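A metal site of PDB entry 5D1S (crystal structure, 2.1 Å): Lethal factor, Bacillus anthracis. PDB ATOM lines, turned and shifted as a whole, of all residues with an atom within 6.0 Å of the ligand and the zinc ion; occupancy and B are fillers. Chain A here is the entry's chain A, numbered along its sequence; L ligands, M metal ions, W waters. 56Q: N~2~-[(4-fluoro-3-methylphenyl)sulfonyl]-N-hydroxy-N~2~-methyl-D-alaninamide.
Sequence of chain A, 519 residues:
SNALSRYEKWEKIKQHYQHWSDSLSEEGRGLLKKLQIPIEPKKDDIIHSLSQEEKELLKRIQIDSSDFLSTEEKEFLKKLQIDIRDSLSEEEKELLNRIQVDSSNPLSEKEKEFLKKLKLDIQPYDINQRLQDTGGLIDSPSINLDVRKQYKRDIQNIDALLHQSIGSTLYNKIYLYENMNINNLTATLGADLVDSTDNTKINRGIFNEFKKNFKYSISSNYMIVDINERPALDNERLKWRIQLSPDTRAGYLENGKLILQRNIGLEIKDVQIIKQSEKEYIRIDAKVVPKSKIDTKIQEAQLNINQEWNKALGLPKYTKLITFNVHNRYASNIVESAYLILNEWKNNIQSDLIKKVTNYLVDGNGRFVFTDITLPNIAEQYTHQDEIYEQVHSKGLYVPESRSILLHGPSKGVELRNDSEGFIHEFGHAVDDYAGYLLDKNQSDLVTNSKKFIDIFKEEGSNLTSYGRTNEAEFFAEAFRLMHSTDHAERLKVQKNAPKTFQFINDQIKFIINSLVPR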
ATOM      1  N   SER A  66       1.171  -8.768  28.606  1.00  0.00           N
ATOM      2  CA  SER A  66       1.900  -8.109  27.512  1.00  0.00           C
ATOM      3  C   SER A  66       1.004  -7.670  26.354  1.00  0.00           C
ATOM      4  O   SER A  66      -0.051  -8.242  26.117  1.00  0.00           O
ATOM      5  CB  SER A  66       3.006  -9.033  26.983  1.00  0.00           C
ATOM      6  OG  SER A  66       4.005  -9.226  27.976  1.00  0.00           O
ATOM      7  N   ASP A  67       1.450  -6.633  25.647  1.00  0.00           N
ATOM      8  CA  ASP A  67       0.785  -6.146  24.432  1.00  0.00           C
ATOM      9  C   ASP A  67       1.274  -6.874  23.211  1.00  0.00           C
ATOM     10  O   ASP A  67       0.669  -6.806  22.144  1.00  0.00           O
ATOM     11  CB  ASP A  67       1.029  -4.646  24.221  1.00  0.00           C
ATOM     12  CG  ASP A  67       0.448  -3.797  25.317  1.00  0.00           C
ATOM     13  OD1 ASP A  67      -0.383  -4.321  26.086  1.00  0.00           O
ATOM     14  OD2 ASP A  67       0.813  -2.598  25.409  1.00  0.00           O
ATOM     15  N   VAL A 392       5.571  -3.972  16.780  1.00  0.00           N
ATOM     16  CA  VAL A 392       4.499  -4.565  17.568  1.00  0.00           C
ATOM     17  C   VAL A 392       3.726  -5.578  16.742  1.00  0.00           C
ATOM     18  O   VAL A 392       3.309  -5.286  15.631  1.00  0.00           O
ATOM     19  CB  VAL A 392       3.478  -3.506  18.088  1.00  0.00           C
ATOM     20  CG1 VAL A 392       2.294  -4.177  18.750  1.00  0.00           C
ATOM     21  CG2 VAL A 392       4.145  -2.525  19.065  1.00  0.00           C
ATOM     22  N   SER A 394       0.154  -7.615  17.065  1.00  0.00           N
ATOM     23  CA  SER A 394      -1.062  -7.599  17.875  1.00  0.00           C
ATOM     24  C   SER A 394      -2.281  -7.759  16.970  1.00  0.00           C
ATOM     25  O   SER A 394      -2.139  -7.851  15.763  1.00  0.00           O
ATOM     26  CB  SER A 394      -1.156  -6.285  18.680  1.00  0.00           C
ATOM     27  OG  SER A 394      -1.261  -5.145  17.839  1.00  0.00           O
ATOM     28  N   LYS A 395      -3.487  -7.765  17.548  1.00  0.00           N
ATOM     29  CA  LYS A 395      -4.703  -7.908  16.763  1.00  0.00           C
ATOM     30  C   LYS A 395      -4.892  -6.688  15.864  1.00  0.00           C
ATOM     31  O   LYS A 395      -5.311  -6.807  14.703  1.00  0.00           O
ATOM     32  CB  LYS A 395      -5.936  -8.102  17.690  1.00  0.00           C
ATOM     33  CG  LYS A 395      -7.286  -7.809  17.025  1.00  0.00           C
ATOM     34  CD  LYS A 395      -7.556  -8.702  15.791  1.00  0.00           C
ATOM     35  CE  LYS A 395      -8.009 -10.079  16.179  1.00  0.00           C
ATOM     36  NZ  LYS A 395      -8.123 -11.059  15.040  1.00  0.00           N
ATOM     37  N   GLY A 396      -4.561  -5.526  16.412  1.00  0.00           N
ATOM     38  CA  GLY A 396      -4.810  -4.278  15.729  1.00  0.00           C
ATOM     39  C   GLY A 396      -3.847  -3.173  16.121  1.00  0.00           C
ATOM     40  O   GLY A 396      -3.224  -3.204  17.178  1.00  0.00           O
ATOM     41  N   LEU A 397      -3.736  -2.172  15.241  1.00  0.00           N
ATOM     42  CA  LEU A 397      -2.745  -1.131  15.398  1.00  0.00           C
ATOM     43  C   LEU A 397      -3.166   0.105  14.605  1.00  0.00           C
ATOM     44  O   LEU A 397      -3.694  -0.006  13.512  1.00  0.00           O
ATOM     45  CB  LEU A 397      -1.363  -1.632  14.928  1.00  0.00           C
ATOM     46  CG  LEU A 397      -0.094  -0.984  15.496  1.00  0.00           C
ATOM     47  CD1 LEU A 397       0.062  -1.301  16.976  1.00  0.00           C
ATOM     48  CD2 LEU A 397       1.190  -1.414  14.751  1.00  0.00           C
ATOM     49  N   TYR A 398      -2.933   1.272  15.187  1.00  0.00           N
ATOM     50  CA  TYR A 398      -2.996   2.498  14.408  1.00  0.00           C
ATOM     51  C   TYR A 398      -1.619   3.100  14.358  1.00  0.00           C
ATOM     52  O   TYR A 398      -0.972   3.256  15.388  1.00  0.00           O
ATOM     53  CB  TYR A 398      -3.967   3.518  15.015  1.00  0.00           C
ATOM     54  CG  TYR A 398      -3.971   4.831  14.271  1.00  0.00           C
ATOM     55  CD1 TYR A 398      -4.529   4.923  13.010  1.00  0.00           C
ATOM     56  CD2 TYR A 398      -3.416   5.984  14.831  1.00  0.00           C
ATOM     57  CE1 TYR A 398      -4.555   6.124  12.324  1.00  0.00           C
ATOM     58  CE2 TYR A 398      -3.439   7.207  14.138  1.00  0.00           C
ATOM     59  CZ  TYR A 398      -4.013   7.248  12.888  1.00  0.00           C
ATOM     60  OH  TYR A 398      -4.048   8.414  12.166  1.00  0.00           O
ATOM     61  N   LYS A 412      -6.073 -13.199  18.390  1.00  0.00           N
ATOM     62  CA  LYS A 412      -7.120 -12.743  19.283  1.00  0.00           C
ATOM     63  C   LYS A 412      -6.611 -11.563  20.088  1.00  0.00           C
ATOM     64  O   LYS A 412      -5.448 -11.537  20.494  1.00  0.00           O
ATOM     65  CB  LYS A 412      -7.594 -13.847  20.219  1.00  0.00           C
ATOM     66  CG  LYS A 412      -8.762 -13.443  21.127  1.00  0.00           C
ATOM     67  CD  LYS A 412      -8.894 -14.359  22.334  1.00  0.00           C
ATOM     68  CE  LYS A 412      -7.677 -14.264  23.244  1.00  0.00           C
ATOM     69  NZ  LYS A 412      -7.759 -15.168  24.435  1.00  0.00           N
ATOM     70  N   GLY A 413      -7.482 -10.585  20.323  1.00  0.00           N
ATOM     71  CA  GLY A 413      -7.104  -9.403  21.073  1.00  0.00           C
ATOM     72  C   GLY A 413      -7.349  -9.526  22.564  1.00  0.00           C
ATOM     73  O   GLY A 413      -8.172 -10.330  23.013  1.00  0.00           O
ATOM     74  N   VAL A 414      -6.612  -8.728  23.330  1.00  0.00           N
ATOM     75  CA  VAL A 414      -6.815  -8.620  24.771  1.00  0.00           C
ATOM     76  C   VAL A 414      -8.266  -8.251  25.096  1.00  0.00           C
ATOM     77  O   VAL A 414      -8.706  -7.148  24.772  1.00  0.00           O
ATOM     78  CB  VAL A 414      -5.901  -7.557  25.389  1.00  0.00           C
ATOM     79  CG1 VAL A 414      -6.058  -7.547  26.908  1.00  0.00           C
ATOM     80  CG2 VAL A 414      -4.449  -7.794  24.979  1.00  0.00           C
ATOM     81  N   GLU A 415      -8.976  -9.180  25.721  1.00  0.00           N
ATOM     82  CA  GLU A 415     -10.360  -8.956  26.172  1.00  0.00           C
ATOM     83  C   GLU A 415     -11.232  -8.333  25.079  1.00  0.00           C
ATOM     84  O   GLU A 415     -11.879  -7.297  25.284  1.00  0.00           O
ATOM     85  CB  GLU A 415     -10.372  -8.082  27.419  1.00  0.00           C
ATOM     86  N   LEU A 416     -11.227  -8.972  23.919  1.00  0.00           N
ATOM     87  CA  LEU A 416     -11.926  -8.487  22.730  1.00  0.00           C
ATOM     88  C   LEU A 416     -12.878  -9.544  22.203  1.00  0.00           C
ATOM     89  O   LEU A 416     -12.461 -10.695  21.982  1.00  0.00           O
ATOM     90  CB  LEU A 416     -10.918  -8.101  21.658  1.00  0.00           C
ATOM     91  CG  LEU A 416     -11.369  -7.166  20.541  1.00  0.00           C
ATOM     92  CD1 LEU A 416     -11.843  -5.862  21.150  1.00  0.00           C
ATOM     93  CD2 LEU A 416     -10.200  -6.934  19.590  1.00  0.00           C
ATOM     94  N   GLU A 421     -14.976  -4.982  16.822  1.00  0.00           N
ATOM     95  CA  GLU A 421     -14.728  -4.117  17.978  1.00  0.00           C
ATOM     96  C   GLU A 421     -13.266  -3.683  17.982  1.00  0.00           C
ATOM     97  O   GLU A 421     -12.962  -2.526  18.308  1.00  0.00           O
ATOM     98  CB  GLU A 421     -15.118  -4.837  19.267  1.00  0.00           C
ATOM     99  CG  GLU A 421     -16.649  -4.997  19.387  1.00  0.00           C
ATOM    100  CD  GLU A 421     -17.087  -5.665  20.686  1.00  0.00           C
ATOM    101  OE1 GLU A 421     -16.287  -6.425  21.280  1.00  0.00           O
ATOM    102  OE2 GLU A 421     -18.237  -5.409  21.119  1.00  0.00           O
ATOM    103  N   GLY A 422     -12.374  -4.581  17.570  1.00  0.00           N
ATOM    104  CA  GLY A 422     -10.975  -4.241  17.428  1.00  0.00           C
ATOM    105  C   GLY A 422     -10.773  -3.085  16.479  1.00  0.00           C
ATOM    106  O   GLY A 422     -10.030  -2.140  16.783  1.00  0.00           O
ATOM    107  N   PHE A 423     -11.470  -3.124  15.355  1.00  0.00           N
ATOM    108  CA  PHE A 423     -11.341  -2.079  14.361  1.00  0.00           C
ATOM    109  C   PHE A 423     -11.824  -0.735  14.903  1.00  0.00           C
ATOM    110  O   PHE A 423     -11.220   0.305  14.624  1.00  0.00           O
ATOM    111  CB  PHE A 423     -12.098  -2.436  13.093  1.00  0.00           C
ATOM    112  CG  PHE A 423     -11.844  -1.501  11.942  1.00  0.00           C
ATOM    113  CD1 PHE A 423     -10.766  -1.709  11.092  1.00  0.00           C
ATOM    114  CD2 PHE A 423     -12.679  -0.422  11.717  1.00  0.00           C
ATOM    115  CE1 PHE A 423     -10.532  -0.843  10.038  1.00  0.00           C
ATOM    116  CE2 PHE A 423     -12.448   0.431  10.681  1.00  0.00           C
ATOM    117  CZ  PHE A 423     -11.388   0.229   9.843  1.00  0.00           C
ATOM    118  N   HIS A 425     -11.828   0.271  17.962  1.00  0.00           N
ATOM    119  CA  HIS A 425     -10.785   0.756  18.855  1.00  0.00           C
ATOM    120  C   HIS A 425      -9.686   1.491  18.075  1.00  0.00           C
ATOM    121  O   HIS A 425      -9.275   2.612  18.445  1.00  0.00           O
ATOM    122  CB  HIS A 425     -10.221  -0.412  19.676  1.00  0.00           C
ATOM    123  CG  HIS A 425      -8.942  -0.111  20.388  1.00  0.00           C
ATOM    124  ND1 HIS A 425      -8.834  -0.125  21.764  1.00  0.00           N
ATOM    125  CD2 HIS A 425      -7.685   0.142  19.927  1.00  0.00           C
ATOM    126  CE1 HIS A 425      -7.581   0.123  22.112  1.00  0.00           C
ATOM    127  NE2 HIS A 425      -6.867   0.304  21.019  1.00  0.00           N
ATOM    128  N   GLU A 426      -9.226   0.878  16.987  1.00  0.00           N
ATOM    129  CA  GLU A 426      -8.202   1.508  16.149  1.00  0.00           C
ATOM    130  C   GLU A 426      -8.726   2.789  15.538  1.00  0.00           C
ATOM    131  O   GLU A 426      -8.017   3.760  15.427  1.00  0.00           O
ATOM    132  CB  GLU A 426      -7.747   0.558  15.034  1.00  0.00           C
ATOM    133  CG  GLU A 426      -7.376  -0.834  15.532  1.00  0.00           C
ATOM    134  CD  GLU A 426      -6.271  -0.819  16.560  1.00  0.00           C
ATOM    135  OE1 GLU A 426      -6.188  -1.774  17.346  1.00  0.00           O
ATOM    136  OE2 GLU A 426      -5.479   0.144  16.568  1.00  0.00           O
ATOM    137  N   HIS A 429      -8.184   5.518  17.887  1.00  0.00           N
ATOM    138  CA  HIS A 429      -6.864   6.111  17.831  1.00  0.00           C
ATOM    139  C   HIS A 429      -6.804   7.162  16.747  1.00  0.00           C
ATOM    140  O   HIS A 429      -6.203   8.233  16.909  1.00  0.00           O
ATOM    141  CB  HIS A 429      -5.793   5.030  17.573  1.00  0.00           C
ATOM    142  CG  HIS A 429      -5.466   4.202  18.769  1.00  0.00           C
ATOM    143  ND1 HIS A 429      -5.205   4.755  20.005  1.00  0.00           N
ATOM    144  CD2 HIS A 429      -5.339   2.863  18.915  1.00  0.00           C
ATOM    145  CE1 HIS A 429      -4.923   3.781  20.864  1.00  0.00           C
ATOM    146  NE2 HIS A 429      -5.014   2.629  20.235  1.00  0.00           N
ATOM    147  N   TYR A 467      -7.432  -3.206  30.212  1.00  0.00           N
ATOM    148  CA  TYR A 467      -6.419  -2.828  29.228  1.00  0.00           C
ATOM    149  C   TYR A 467      -6.330  -1.314  29.131  1.00  0.00           C
ATOM    150  O   TYR A 467      -5.270  -0.767  28.861  1.00  0.00           O
ATOM    151  CB  TYR A 467      -6.705  -3.420  27.842  1.00  0.00           C
ATOM    152  CG  TYR A 467      -5.697  -2.931  26.834  1.00  0.00           C
ATOM    153  CD1 TYR A 467      -4.360  -3.273  26.945  1.00  0.00           C
ATOM    154  CD2 TYR A 467      -6.078  -2.097  25.791  1.00  0.00           C
ATOM    155  CE1 TYR A 467      -3.416  -2.803  26.029  1.00  0.00           C
ATOM    156  CE2 TYR A 467      -5.140  -1.629  24.867  1.00  0.00           C
ATOM    157  CZ  TYR A 467      -3.811  -1.985  24.988  1.00  0.00           C
ATOM    158  OH  TYR A 467      -2.891  -1.511  24.076  1.00  0.00           O
ATOM    159  N   ALA A 473      -3.682   7.268  25.535  1.00  0.00           N
ATOM    160  CA  ALA A 473      -4.112   6.929  24.195  1.00  0.00           C
ATOM    161  C   ALA A 473      -5.002   5.680  24.205  1.00  0.00           C
ATOM    162  O   ALA A 473      -5.993   5.614  23.474  1.00  0.00           O
ATOM    163  CB  ALA A 473      -2.890   6.710  23.265  1.00  0.00           C
ATOM    164  N   GLU A 474      -4.644   4.688  25.010  1.00  0.00           N
ATOM    165  CA  GLU A 474      -5.381   3.435  25.033  1.00  0.00           C
ATOM    166  C   GLU A 474      -6.688   3.629  25.816  1.00  0.00           C
ATOM    167  O   GLU A 474      -7.740   3.109  25.423  1.00  0.00           O
ATOM    168  CB  GLU A 474      -4.541   2.316  25.647  1.00  0.00           C
ATOM    169  CG  GLU A 474      -3.179   2.098  24.994  1.00  0.00           C
ATOM    170  CD  GLU A 474      -3.249   1.617  23.546  1.00  0.00           C
ATOM    171  OE1 GLU A 474      -4.359   1.383  23.035  1.00  0.00           O
ATOM    172  OE2 GLU A 474      -2.181   1.467  22.919  1.00  0.00           O
ATOM    173  N   ALA A 477      -9.113   5.191  23.504  1.00  0.00           N
ATOM    174  CA  ALA A 477      -9.523   4.234  22.480  1.00  0.00           C
ATOM    175  C   ALA A 477     -10.501   3.196  23.027  1.00  0.00           C
ATOM    176  O   ALA A 477     -11.482   2.876  22.378  1.00  0.00           O
ATOM    177  CB  ALA A 477      -8.301   3.536  21.848  1.00  0.00           C
ATOM    178  N   GLU A 478     -10.206   2.672  24.211  1.00  0.00           N
ATOM    179  CA  GLU A 478     -11.108   1.747  24.864  1.00  0.00           C
ATOM    180  C   GLU A 478     -12.451   2.421  25.185  1.00  0.00           C
ATOM    181  O   GLU A 478     -13.517   1.872  24.912  1.00  0.00           O
ATOM    182  CB  GLU A 478     -10.462   1.162  26.117  1.00  0.00           C
ATOM    183  CG  GLU A 478      -9.452   0.044  25.812  1.00  0.00           C
ATOM    184  CD  GLU A 478     -10.116  -1.176  25.198  1.00  0.00           C
ATOM    185  OE1 GLU A 478     -10.250  -2.198  25.896  1.00  0.00           O
ATOM    186  OE2 GLU A 478     -10.534  -1.103  24.014  1.00  0.00           O
ATOM    187  N   ARG A 481     -14.284   2.810  22.029  1.00  0.00           N
ATOM    188  CA  ARG A 481     -14.822   1.537  21.588  1.00  0.00           C
ATOM    189  C   ARG A 481     -16.116   1.214  22.323  1.00  0.00           C
ATOM    190  O   ARG A 481     -17.127   0.908  21.705  1.00  0.00           O
ATOM    191  CB  ARG A 481     -13.824   0.416  21.803  1.00  0.00           C
ATOM    192  CG  ARG A 481     -14.428  -0.943  21.586  1.00  0.00           C
ATOM    193  CD  ARG A 481     -13.386  -2.026  21.605  1.00  0.00           C
ATOM    194  NE  ARG A 481     -12.857  -2.258  22.936  1.00  0.00           N
ATOM    195  CZ  ARG A 481     -13.423  -3.049  23.838  1.00  0.00           C
ATOM    196  NH1 ARG A 481     -14.559  -3.680  23.562  1.00  0.00           N
ATOM    197  NH2 ARG A 481     -12.857  -3.215  25.023  1.00  0.00           N
HETATM  198  C1  56Q L   1      -3.016  -3.336  20.601  1.00  0.00           C
HETATM  199  C2  56Q L   1      -3.577  -1.910  20.556  1.00  0.00           C
HETATM  200  O5  56Q L   1      -4.286  -0.251  18.944  1.00  0.00           O
HETATM  201  N6  56Q L   1      -3.708  -4.444  21.321  1.00  0.00           N
HETATM  202  C10 56Q L   1      -6.231  -4.716  20.800  1.00  0.00           C
HETATM  203  C11 56Q L   1      -6.973  -4.838  21.989  1.00  0.00           C
HETATM  204  C12 56Q L   1      -8.230  -4.224  22.094  1.00  0.00           C
HETATM  205  C13 56Q L   1      -8.724  -3.508  21.000  1.00  0.00           C
HETATM  206  C14 56Q L   1      -7.997  -3.394  19.825  1.00  0.00           C
HETATM  207  C15 56Q L   1      -6.748  -4.001  19.723  1.00  0.00           C
HETATM  208  C18 56Q L   1      -3.339  -4.684  22.710  1.00  0.00           C
HETATM  209  C28 56Q L   1      -1.560  -3.206  21.081  1.00  0.00           C
HETATM  210  N4  56Q L   1      -3.796  -1.491  19.316  1.00  0.00           N
HETATM  211  O3  56Q L   1      -3.761  -1.177  21.535  1.00  0.00           O
HETATM  212  S7  56Q L   1      -4.778  -5.406  20.668  1.00  0.00           S
HETATM  213  O8  56Q L   1      -4.875  -6.716  21.269  1.00  0.00           O
HETATM  214  O9  56Q L   1      -4.456  -5.598  19.272  1.00  0.00           O
HETATM  215  F16 56Q L   1      -9.929  -2.925  21.087  1.00  0.00           F
HETATM  216  C17 56Q L   1      -9.060  -4.320  23.356  1.00  0.00           C
HETATM  217 ZN    ZN M   1      -4.694   0.695  20.995  1.00  0.00          ZN
HETATM  218  O   HOH W   1     -10.128  -4.773  26.557  1.00  0.00           O
HETATM  219  O   HOH W   2      -2.188   1.253  18.166  1.00  0.00           O
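Ser 394 touches the ligand. Leu 397 touches the ligand (CA to O5, 3.97 Å). Gly 413 touches the ligand. CD1 of Leu 416 touches F16 of the ligand, at 3.5 Å. O of Gly 422 touches C14 of the ligand (3.9 Å). Glu 478 touches the ligand. NE of Arg 481 touches F16 of the ligand, 3.5 Å away. 15 residues have an atom within 4 Å of the ligand: Ser 394, Lys 395, Gly 396, Leu 397, Gly 413, Val 414, Leu 416, Gly 422, His 425, Glu 426, His 429, Tyr 467, Glu 474, Glu 478 and Arg 481. Along chain A the residues within 4 Å of the ligand span positions 394 to 481. The nearest printed residue that does not touch the ligand is Glu 421 (4.1 Å).
A ring nitrogen (NE2) of His 429 is bound to the zinc ion (2.1 Å). An oxygen (O3) of the ligand is bound to the zinc ion (2.2 Å). The zinc ion is bound by OE1 of Glu 474, 2.2 Å away. The zinc ion is bound by NE2 of His 425 (2.2 Å). O5 of the ligand is bound to the zinc ion (2.3 Å).
The side-chain carboxylate of Glu 474 lies close to the side-chain hydroxyl of Tyr 467. ND1 of His 425 sits at hydrogen-bond distance from OE2 of Glu 478 (3.0 Å). N of Leu 397 lies close to OE2 of Glu 426 (3.2 Å). The side-chain carboxylate of Glu 426 sits at hydrogen-bond distance from the backbone NH of Tyr 398 (3.1 Å). The side-chain hydroxyl (OG) of Ser 394 lies within hydrogen-bond range of the backbone carbonyl oxygen (O) of Gly 396 (2.8 Å). NE of Arg 481 is in salt-bridge range of OE2 of Glu 478. NH1 of Arg 481 is in salt-bridge range of OE1 of Glu 421.
Within 4 Å of the zinc ion: His 425, His 429 and Glu 474. The nearest printed residue that does not touch the zinc ion is Tyr 467 (4.2 Å).
Water W2 lies within hydrogen-bond range of N of Tyr 398 (3.1 Å) and N4 of the ligand (3.4 Å).
The side-chain carboxylate (OE1) of Glu 426 is in hydrogen-bond range of a nitrogen (N4) of the ligand. The side-chain hydroxyl of Tyr 467 sits close to an oxygen (O3) of the ligand, 2.7 Å away. N of Gly 396 is in hydrogen-bond range of O9 of the ligand, at 2.9 Å. The backbone carbonyl oxygen of Gly 396 lies within hydrogen-bond range of a nitrogen (N4) of the ligand (2.8 Å). The backbone NH of Lys 395 sits at hydrogen-bond distance from an oxygen (O9) of the ligand (2.9 Å). O8 of the ligand sits at hydrogen-bond distance from N of Val 414 (3.4 Å).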
